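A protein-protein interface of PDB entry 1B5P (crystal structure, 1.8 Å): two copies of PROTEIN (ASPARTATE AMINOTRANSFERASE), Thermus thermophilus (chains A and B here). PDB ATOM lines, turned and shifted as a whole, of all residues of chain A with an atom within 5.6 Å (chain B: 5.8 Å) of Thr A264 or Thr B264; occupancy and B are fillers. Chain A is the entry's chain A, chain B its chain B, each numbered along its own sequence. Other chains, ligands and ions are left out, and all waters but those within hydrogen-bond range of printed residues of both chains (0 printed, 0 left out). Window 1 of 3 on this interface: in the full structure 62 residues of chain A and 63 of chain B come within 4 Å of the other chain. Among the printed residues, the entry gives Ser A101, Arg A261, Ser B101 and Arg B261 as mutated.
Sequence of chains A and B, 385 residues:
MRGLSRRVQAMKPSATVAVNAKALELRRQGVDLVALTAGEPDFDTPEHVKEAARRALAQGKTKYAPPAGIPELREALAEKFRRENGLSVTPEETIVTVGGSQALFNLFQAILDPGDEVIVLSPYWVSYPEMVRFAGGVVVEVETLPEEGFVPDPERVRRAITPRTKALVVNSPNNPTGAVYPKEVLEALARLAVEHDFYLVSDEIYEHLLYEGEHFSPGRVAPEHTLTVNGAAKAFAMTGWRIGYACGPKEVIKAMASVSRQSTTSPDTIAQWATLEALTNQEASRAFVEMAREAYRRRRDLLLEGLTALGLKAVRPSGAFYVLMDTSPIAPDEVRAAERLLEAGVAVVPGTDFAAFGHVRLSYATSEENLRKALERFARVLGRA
NE of Arg B242 lies close to O of Ser A266, 3.3 Å away. OG of Ser B101 is in hydrogen-bond range of O of Ser A263. NH2 of Arg A242 is in hydrogen-bond range of O of Thr B264 (3.0 Å). The backbone carbonyl oxygen of Ser B263 sits at hydrogen-bond distance from the backbone NH of Gln A102, 3.1 Å away. OG1 of Thr A265 is in hydrogen-bond range of OG of Ser B101, at 3.1 Å. OG of Ser A101 lies within hydrogen-bond range of OG1 of Thr B265. The guanidinium group (NE) of Arg A242 lies close to the backbone carbonyl oxygen (O) of Ser B266. The side-chain hydroxyl (OG1) of Thr A265 lies within hydrogen-bond range of the guanidinium group (NH2) of Arg B242, 3.4 Å away. The backbone carbonyl oxygen (O) of Ser B263 lies within hydrogen-bond range of the side-chain hydroxyl (OG) of Ser A101 (2.7 Å). The backbone NH of Gln B102 sits at hydrogen-bond distance from the backbone carbonyl oxygen of Ser A263 (3.0 Å). The guanidinium group (NH2) of Arg B242 sits at hydrogen-bond distance from the backbone carbonyl oxygen (O) of Thr A264 (2.9 Å).
The backbone NH of Val A98 is in hydrogen-bond range of the side-chain amide oxygen of Gln A102 (2.8 Å). The side-chain amide nitrogen (NE2) of Gln B102 sits at hydrogen-bond distance from the side-chain hydroxyl (OG1) of Thr B264 (2.9 Å). N of Thr A265 sits at hydrogen-bond distance from O of Ser A260 (2.8 Å). The backbone NH (N) of Gly B99 is in hydrogen-bond range of the backbone carbonyl oxygen (O) of Arg B242 (3.3 Å). O of Ser A260 is in hydrogen-bond range of OG of Ser A263. The backbone NH (N) of Gly A99 sits close to the backbone carbonyl oxygen (O) of Arg A242 (3.4 Å).
Among the printed residues, pairs that only touch across the chains: Val A98 with Thr B264 (3.6 Å), Ser A101 with Thr B264 (3.7 Å), Arg A242 with Thr B265 (3.7 Å), Arg A242 with Pro B267 (3.9 Å), Thr A264 with Val B98 (3.8 Å), Thr A264 with Ser B101 (3.7 Å), Thr A264 with Thr B264 (3.9 Å) and Pro A267 with Arg B242 (3.8 Å).
Of the printed residues of chain B, Thr A264 touches Val B98 (3.8 Å), Ser B101 (3.7 Å), Arg B242 (2.9 Å) and Thr B264 (3.9 Å). Thr B264 touches just these residues of chain A: Val A98 (3.6 Å), Ser A101 (3.7 Å), Arg A242 (3.0 Å) and Thr A264 (3.9 Å). Of the printed residues of chain B, Arg A242 touches Thr B264, Thr B265, Ser B266 and Pro B267. Printed residues of chain B within 4 Å of Val A98: Thr B264 (3.6 Å). Printed residues of chain B within 4 Å of Gln A102: Ser B263 (3.1 Å). Ser B260 touches none of the printed residues of chain A. The nearest residue of chain A that does not touch Thr B264 is Gln A102 (4.4 Å).
Of the 14 printed residues of chain A, 9 touch a printed residue of chain B. Hydrophobic or aromatic side chains of chain A that line the printed part of chain B: Val A98. Along chain A the printed residues that touch a printed residue of chain B span positions 98 to 267.
Ser A101 touches Thr B265, and with the chains exchanged Thr A265 touches Ser B101. Gln A102 touches Ser B263, and with the chains exchanged Ser A263 touches Gln B102. Arg A242 touches Thr B264, and with the chains exchanged Thr A264 touches Arg B242. Thr B264 touches its own counterpart, Thr A264. 14 positions are printed for both chains.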
ATOM      1  N   VAL A  98      12.712  26.290  14.057  1.00  0.00           N
ATOM      2  CA  VAL A  98      11.639  25.901  14.975  1.00  0.00           C
ATOM      3  C   VAL A  98      12.178  26.129  16.390  1.00  0.00           C
ATOM      4  O   VAL A  98      12.678  25.218  17.052  1.00  0.00           O
ATOM      5  CB  VAL A  98      11.228  24.416  14.752  1.00  0.00           C
ATOM      6  CG1 VAL A  98      10.130  24.008  15.722  1.00  0.00           C
ATOM      7  CG2 VAL A  98      10.759  24.223  13.312  1.00  0.00           C
ATOM      8  N   GLY A  99      12.071  27.382  16.815  1.00  0.00           N
ATOM      9  CA  GLY A  99      12.552  27.806  18.106  1.00  0.00           C
ATOM     10  C   GLY A  99      14.040  28.082  18.025  1.00  0.00           C
ATOM     11  O   GLY A  99      14.709  27.701  17.061  1.00  0.00           O
ATOM     12  N   SER A 101      15.857  26.870  19.943  1.00  0.00           N
ATOM     13  CA  SER A 101      16.459  25.587  20.261  1.00  0.00           C
ATOM     14  C   SER A 101      16.876  24.852  18.993  1.00  0.00           C
ATOM     15  O   SER A 101      17.933  24.224  18.971  1.00  0.00           O
ATOM     16  CB  SER A 101      15.543  24.720  21.131  1.00  0.00           C
ATOM     17  OG  SER A 101      14.406  24.281  20.415  1.00  0.00           O
ATOM     18  N   GLN A 102      16.101  24.976  17.915  1.00  0.00           N
ATOM     19  CA  GLN A 102      16.474  24.279  16.681  1.00  0.00           C
ATOM     20  C   GLN A 102      17.666  24.933  16.005  1.00  0.00           C
ATOM     21  O   GLN A 102      18.441  24.269  15.332  1.00  0.00           O
ATOM     22  CB  GLN A 102      15.325  24.153  15.682  1.00  0.00           C
ATOM     23  CG  GLN A 102      15.681  23.112  14.624  1.00  0.00           C
ATOM     24  CD  GLN A 102      14.816  23.148  13.392  1.00  0.00           C
ATOM     25  OE1 GLN A 102      14.260  24.180  13.025  1.00  0.00           O
ATOM     26  NE2 GLN A 102      14.736  22.017  12.719  1.00  0.00           N
ATOM     27  N   ARG A 242       7.008  28.424  18.353  1.00  0.00           N
ATOM     28  CA  ARG A 242       8.208  27.778  17.820  1.00  0.00           C
ATOM     29  C   ARG A 242       8.875  28.463  16.616  1.00  0.00           C
ATOM     30  O   ARG A 242       8.975  27.888  15.524  1.00  0.00           O
ATOM     31  CB  ARG A 242       7.950  26.286  17.525  1.00  0.00           C
ATOM     32  CG  ARG A 242       7.149  25.531  18.592  1.00  0.00           C
ATOM     33  CD  ARG A 242       7.753  25.613  19.998  1.00  0.00           C
ATOM     34  NE  ARG A 242       9.166  25.247  20.005  1.00  0.00           N
ATOM     35  CZ  ARG A 242      10.132  26.031  20.480  1.00  0.00           C
ATOM     36  NH1 ARG A 242       9.848  27.221  20.998  1.00  0.00           N
ATOM     37  NH2 ARG A 242      11.392  25.646  20.401  1.00  0.00           N
ATOM     38  N   VAL A 259      20.127  21.067   7.062  1.00  0.00           N
ATOM     39  CA  VAL A 259      19.746  20.195   8.175  1.00  0.00           C
ATOM     40  C   VAL A 259      18.232  20.320   8.365  1.00  0.00           C
ATOM     41  O   VAL A 259      17.565  19.337   8.673  1.00  0.00           O
ATOM     42  CB  VAL A 259      20.463  20.588   9.516  1.00  0.00           C
ATOM     43  CG1 VAL A 259      19.981  19.695  10.663  1.00  0.00           C
ATOM     44  CG2 VAL A 259      21.974  20.459   9.377  1.00  0.00           C
ATOM     45  N   SER A 260      17.700  21.529   8.186  1.00  0.00           N
ATOM     46  CA  SER A 260      16.262  21.753   8.322  1.00  0.00           C
ATOM     47  C   SER A 260      15.503  21.035   7.219  1.00  0.00           C
ATOM     48  O   SER A 260      14.499  20.370   7.472  1.00  0.00           O
ATOM     49  CB  SER A 260      15.930  23.242   8.273  1.00  0.00           C
ATOM     50  OG  SER A 260      16.249  23.858   9.509  1.00  0.00           O
ATOM     51  N   ARG A 261      16.003  21.158   5.997  1.00  0.00           N
ATOM     52  CA  ARG A 261      15.372  20.528   4.846  1.00  0.00           C
ATOM     53  C   ARG A 261      15.227  19.013   5.008  1.00  0.00           C
ATOM     54  O   ARG A 261      14.279  18.417   4.502  1.00  0.00           O
ATOM     55  CB  ARG A 261      16.146  20.868   3.572  1.00  0.00           C
ATOM     56  CG  ARG A 261      15.630  20.150   2.346  1.00  0.00           C
ATOM     57  CD  ARG A 261      16.078  20.787   1.041  1.00  0.00           C
ATOM     58  NE  ARG A 261      17.483  21.194   0.992  1.00  0.00           N
ATOM     59  CZ  ARG A 261      18.532  20.416   1.280  1.00  0.00           C
ATOM     60  NH1 ARG A 261      18.367  19.148   1.665  1.00  0.00           N
ATOM     61  NH2 ARG A 261      19.764  20.909   1.152  1.00  0.00           N
ATOM     62  N   GLN A 262      16.154  18.403   5.737  1.00  0.00           N
ATOM     63  CA  GLN A 262      16.116  16.967   5.954  1.00  0.00           C
ATOM     64  C   GLN A 262      15.488  16.582   7.275  1.00  0.00           C
ATOM     65  O   GLN A 262      15.534  15.408   7.666  1.00  0.00           O
ATOM     66  CB  GLN A 262      17.509  16.387   5.991  1.00  0.00           C
ATOM     67  CG  GLN A 262      18.365  16.575   4.803  1.00  0.00           C
ATOM     68  CD  GLN A 262      19.732  16.032   5.097  1.00  0.00           C
ATOM     69  OE1 GLN A 262      20.733  16.594   4.678  1.00  0.00           O
ATOM     70  NE2 GLN A 262      19.783  14.968   5.897  1.00  0.00           N
ATOM     71  N   SER A 263      14.953  17.551   8.004  1.00  0.00           N
ATOM     72  CA  SER A 263      14.372  17.208   9.287  1.00  0.00           C
ATOM     73  C   SER A 263      12.967  17.753   9.496  1.00  0.00           C
ATOM     74  O   SER A 263      12.011  16.989   9.494  1.00  0.00           O
ATOM     75  CB  SER A 263      15.318  17.625  10.426  1.00  0.00           C
ATOM     76  OG  SER A 263      15.682  18.997  10.338  1.00  0.00           O
ATOM     77  N   THR A 264      12.839  19.072   9.596  1.00  0.00           N
ATOM     78  CA  THR A 264      11.543  19.699   9.823  1.00  0.00           C
ATOM     79  C   THR A 264      10.940  20.316   8.565  1.00  0.00           C
ATOM     80  O   THR A 264       9.772  20.721   8.566  1.00  0.00           O
ATOM     81  CB  THR A 264      11.656  20.829  10.847  1.00  0.00           C
ATOM     82  OG1 THR A 264      12.755  21.672  10.489  1.00  0.00           O
ATOM     83  CG2 THR A 264      11.859  20.287  12.243  1.00  0.00           C
ATOM     84  N   THR A 265      11.743  20.361   7.499  1.00  0.00           N
ATOM     85  CA  THR A 265      11.391  20.976   6.215  1.00  0.00           C
ATOM     86  C   THR A 265      11.440  22.520   6.279  1.00  0.00           C
ATOM     87  O   THR A 265      12.209  23.127   5.547  1.00  0.00           O
ATOM     88  CB  THR A 265      10.039  20.477   5.640  1.00  0.00           C
ATOM     89  OG1 THR A 265      10.069  19.049   5.551  1.00  0.00           O
ATOM     90  CG2 THR A 265       9.835  21.041   4.243  1.00  0.00           C
ATOM     91  N   SER A 266      10.632  23.130   7.152  1.00  0.00           N
ATOM     92  CA  SER A 266      10.584  24.586   7.362  1.00  0.00           C
ATOM     93  C   SER A 266       9.648  24.827   8.541  1.00  0.00           C
ATOM     94  O   SER A 266       8.803  23.984   8.834  1.00  0.00           O
ATOM     95  CB  SER A 266      10.033  25.318   6.132  1.00  0.00           C
ATOM     96  OG  SER A 266      10.113  26.738   6.291  1.00  0.00           O
ATOM     97  N   PRO A 267       9.807  25.951   9.266  1.00  0.00           N
ATOM     98  CA  PRO A 267       8.871  26.140  10.385  1.00  0.00           C
ATOM     99  C   PRO A 267       7.464  26.451   9.869  1.00  0.00           C
ATOM    100  O   PRO A 267       7.289  26.809   8.704  1.00  0.00           O
ATOM    101  CB  PRO A 267       9.448  27.345  11.131  1.00  0.00           C
ATOM    102  CG  PRO A 267      10.903  27.323  10.778  1.00  0.00           C
ATOM    103  CD  PRO A 267      10.903  26.938   9.321  1.00  0.00           C
ATOM    104  N   VAL B  98       7.118  17.766  14.176  1.00  0.00           N
ATOM    105  CA  VAL B  98       7.069  18.905  13.250  1.00  0.00           C
ATOM    106  C   VAL B  98       7.093  18.308  11.835  1.00  0.00           C
ATOM    107  O   VAL B  98       8.125  18.231  11.163  1.00  0.00           O
ATOM    108  CB  VAL B  98       8.255  19.919  13.481  1.00  0.00           C
ATOM    109  CG1 VAL B  98       8.191  21.084  12.492  1.00  0.00           C
ATOM    110  CG2 VAL B  98       8.196  20.465  14.915  1.00  0.00           C
ATOM    111  N   GLY B  99       5.914  17.862  11.426  1.00  0.00           N
ATOM    112  CA  GLY B  99       5.727  17.216  10.144  1.00  0.00           C
ATOM    113  C   GLY B  99       6.118  15.756  10.206  1.00  0.00           C
ATOM    114  O   GLY B  99       6.778  15.315  11.152  1.00  0.00           O
ATOM    115  N   SER B 101       8.026  14.531   8.313  1.00  0.00           N
ATOM    116  CA  SER B 101       9.453  14.531   8.029  1.00  0.00           C
ATOM    117  C   SER B 101      10.251  14.464   9.336  1.00  0.00           C
ATOM    118  O   SER B 101      11.232  13.732   9.410  1.00  0.00           O
ATOM    119  CB  SER B 101       9.872  15.714   7.154  1.00  0.00           C
ATOM    120  OG  SER B 101       9.630  16.959   7.774  1.00  0.00           O
ATOM    121  N   GLN B 102       9.826  15.173  10.384  1.00  0.00           N
ATOM    122  CA  GLN B 102      10.574  15.072  11.638  1.00  0.00           C
ATOM    123  C   GLN B 102      10.394  13.730  12.353  1.00  0.00           C
ATOM    124  O   GLN B 102      11.282  13.314  13.097  1.00  0.00           O
ATOM    125  CB  GLN B 102      10.311  16.224  12.611  1.00  0.00           C
ATOM    126  CG  GLN B 102      11.241  16.117  13.833  1.00  0.00           C
ATOM    127  CD  GLN B 102      10.848  17.012  14.973  1.00  0.00           C
ATOM    128  OE1 GLN B 102       9.665  17.170  15.276  1.00  0.00           O
ATOM    129  NE2 GLN B 102      11.841  17.587  15.642  1.00  0.00           N
ATOM    130  N   ASN B 106      13.751  11.866  13.470  1.00  0.00           N
ATOM    131  CA  ASN B 106      13.947  11.481  14.869  1.00  0.00           C
ATOM    132  C   ASN B 106      14.071   9.982  15.021  1.00  0.00           C
ATOM    133  O   ASN B 106      14.839   9.491  15.844  1.00  0.00           O
ATOM    134  CB  ASN B 106      12.796  11.991  15.755  1.00  0.00           C
ATOM    135  CG  ASN B 106      12.852  13.491  15.986  1.00  0.00           C
ATOM    136  OD1 ASN B 106      13.630  14.203  15.353  1.00  0.00           O
ATOM    137  ND2 ASN B 106      12.015  13.979  16.895  1.00  0.00           N
ATOM    138  N   ARG B 242       2.983  21.973   9.555  1.00  0.00           N
ATOM    139  CA  ARG B 242       4.040  21.147  10.133  1.00  0.00           C
ATOM    140  C   ARG B 242       3.631  20.296  11.347  1.00  0.00           C
ATOM    141  O   ARG B 242       4.167  20.471  12.447  1.00  0.00           O
ATOM    142  CB  ARG B 242       5.265  22.003  10.498  1.00  0.00           C
ATOM    143  CG  ARG B 242       5.654  23.085   9.492  1.00  0.00           C
ATOM    144  CD  ARG B 242       5.976  22.539   8.101  1.00  0.00           C
ATOM    145  NE  ARG B 242       6.882  21.399   8.146  1.00  0.00           N
ATOM    146  CZ  ARG B 242       6.595  20.205   7.618  1.00  0.00           C
ATOM    147  NH1 ARG B 242       5.428  19.990   6.996  1.00  0.00           N
ATOM    148  NH2 ARG B 242       7.463  19.210   7.726  1.00  0.00           N
ATOM    149  N   VAL B 259      14.672  13.107  21.381  1.00  0.00           N
ATOM    150  CA  VAL B 259      15.308  13.845  20.298  1.00  0.00           C
ATOM    151  C   VAL B 259      14.593  15.171  20.084  1.00  0.00           C
ATOM    152  O   VAL B 259      15.243  16.197  19.887  1.00  0.00           O
ATOM    153  CB  VAL B 259      15.353  13.041  18.983  1.00  0.00           C
ATOM    154  CG1 VAL B 259      16.021  13.863  17.887  1.00  0.00           C
ATOM    155  CG2 VAL B 259      16.124  11.744  19.197  1.00  0.00           C
ATOM    156  N   SER B 260      13.256  15.163  20.142  1.00  0.00           N
ATOM    157  CA  SER B 260      12.502  16.404  19.981  1.00  0.00           C
ATOM    158  C   SER B 260      12.821  17.371  21.114  1.00  0.00           C
ATOM    159  O   SER B 260      12.922  18.571  20.895  1.00  0.00           O
ATOM    160  CB  SER B 260      10.996  16.147  19.978  1.00  0.00           C
ATOM    161  OG  SER B 260      10.602  15.425  18.826  1.00  0.00           O
ATOM    162  N   ARG B 261      12.965  16.841  22.320  1.00  0.00           N
ATOM    163  CA  ARG B 261      13.261  17.682  23.471  1.00  0.00           C
ATOM    164  C   ARG B 261      14.556  18.465  23.282  1.00  0.00           C
ATOM    165  O   ARG B 261      14.638  19.636  23.643  1.00  0.00           O
ATOM    166  CB  ARG B 261      13.327  16.849  24.743  1.00  0.00           C
ATOM    167  CG  ARG B 261      13.273  17.684  25.999  1.00  0.00           C
ATOM    168  CD  ARG B 261      13.218  16.797  27.213  1.00  0.00           C
ATOM    169  NE  ARG B 261      14.264  15.785  27.154  1.00  0.00           N
ATOM    170  CZ  ARG B 261      15.564  16.051  27.249  1.00  0.00           C
ATOM    171  NH1 ARG B 261      15.981  17.306  27.418  1.00  0.00           N
ATOM    172  NH2 ARG B 261      16.448  15.066  27.130  1.00  0.00           N
ATOM    173  N   GLN B 262      15.551  17.819  22.685  1.00  0.00           N
ATOM    174  CA  GLN B 262      16.854  18.437  22.433  1.00  0.00           C
ATOM    175  C   GLN B 262      16.977  19.181  21.106  1.00  0.00           C
ATOM    176  O   GLN B 262      18.071  19.642  20.767  1.00  0.00           O
ATOM    177  CB  GLN B 262      17.947  17.376  22.451  1.00  0.00           C
ATOM    178  CG  GLN B 262      17.862  16.392  23.573  1.00  0.00           C
ATOM    179  CD  GLN B 262      18.904  15.319  23.429  1.00  0.00           C
ATOM    180  OE1 GLN B 262      18.579  14.157  23.209  1.00  0.00           O
ATOM    181  NE2 GLN B 262      20.174  15.704  23.530  1.00  0.00           N
ATOM    182  N   SER B 263      15.892  19.262  20.334  1.00  0.00           N
ATOM    183  CA  SER B 263      15.955  19.953  19.053  1.00  0.00           C
ATOM    184  C   SER B 263      14.891  21.018  18.840  1.00  0.00           C
ATOM    185  O   SER B 263      15.183  22.208  18.850  1.00  0.00           O
ATOM    186  CB  SER B 263      15.958  18.939  17.890  1.00  0.00           C
ATOM    187  OG  SER B 263      14.843  18.030  17.971  1.00  0.00           O
ATOM    188  N   THR B 264      13.639  20.586  18.722  1.00  0.00           N
ATOM    189  CA  THR B 264      12.525  21.500  18.471  1.00  0.00           C
ATOM    190  C   THR B 264      11.684  21.828  19.706  1.00  0.00           C
ATOM    191  O   THR B 264      10.872  22.763  19.681  1.00  0.00           O
ATOM    192  CB  THR B 264      11.556  20.865  17.441  1.00  0.00           C
ATOM    193  OG1 THR B 264      11.386  19.481  17.781  1.00  0.00           O
ATOM    194  CG2 THR B 264      12.107  20.992  16.034  1.00  0.00           C
ATOM    195  N   THR B 265      11.927  21.073  20.781  1.00  0.00           N
ATOM    196  CA  THR B 265      11.203  21.140  22.050  1.00  0.00           C
ATOM    197  C   THR B 265       9.817  20.495  21.890  1.00  0.00           C
ATOM    198  O   THR B 265       9.543  19.483  22.525  1.00  0.00           O
ATOM    199  CB  THR B 265      11.139  22.562  22.675  1.00  0.00           C
ATOM    200  OG1 THR B 265      12.474  23.065  22.817  1.00  0.00           O
ATOM    201  CG2 THR B 265      10.517  22.495  24.074  1.00  0.00           C
ATOM    202  N   SER B 266       9.000  21.012  20.973  1.00  0.00           N
ATOM    203  CA  SER B 266       7.660  20.483  20.704  1.00  0.00           C
ATOM    204  C   SER B 266       7.076  21.230  19.511  1.00  0.00           C
ATOM    205  O   SER B 266       7.490  22.352  19.222  1.00  0.00           O
ATOM    206  CB  SER B 266       6.755  20.695  21.925  1.00  0.00           C
ATOM    207  OG  SER B 266       5.480  20.087  21.744  1.00  0.00           O
ATOM    208  N   PRO B 267       6.157  20.599  18.749  1.00  0.00           N
ATOM    209  CA  PRO B 267       5.557  21.288  17.603  1.00  0.00           C
ATOM    210  C   PRO B 267       4.725  22.485  18.088  1.00  0.00           C
ATOM    211  O   PRO B 267       4.327  22.543  19.242  1.00  0.00           O
ATOM    212  CB  PRO B 267       4.641  20.219  16.987  1.00  0.00           C
ATOM    213  CG  PRO B 267       5.325  18.947  17.331  1.00  0.00           C
ATOM    214  CD  PRO B 267       5.804  19.162  18.745  1.00  0.00           C
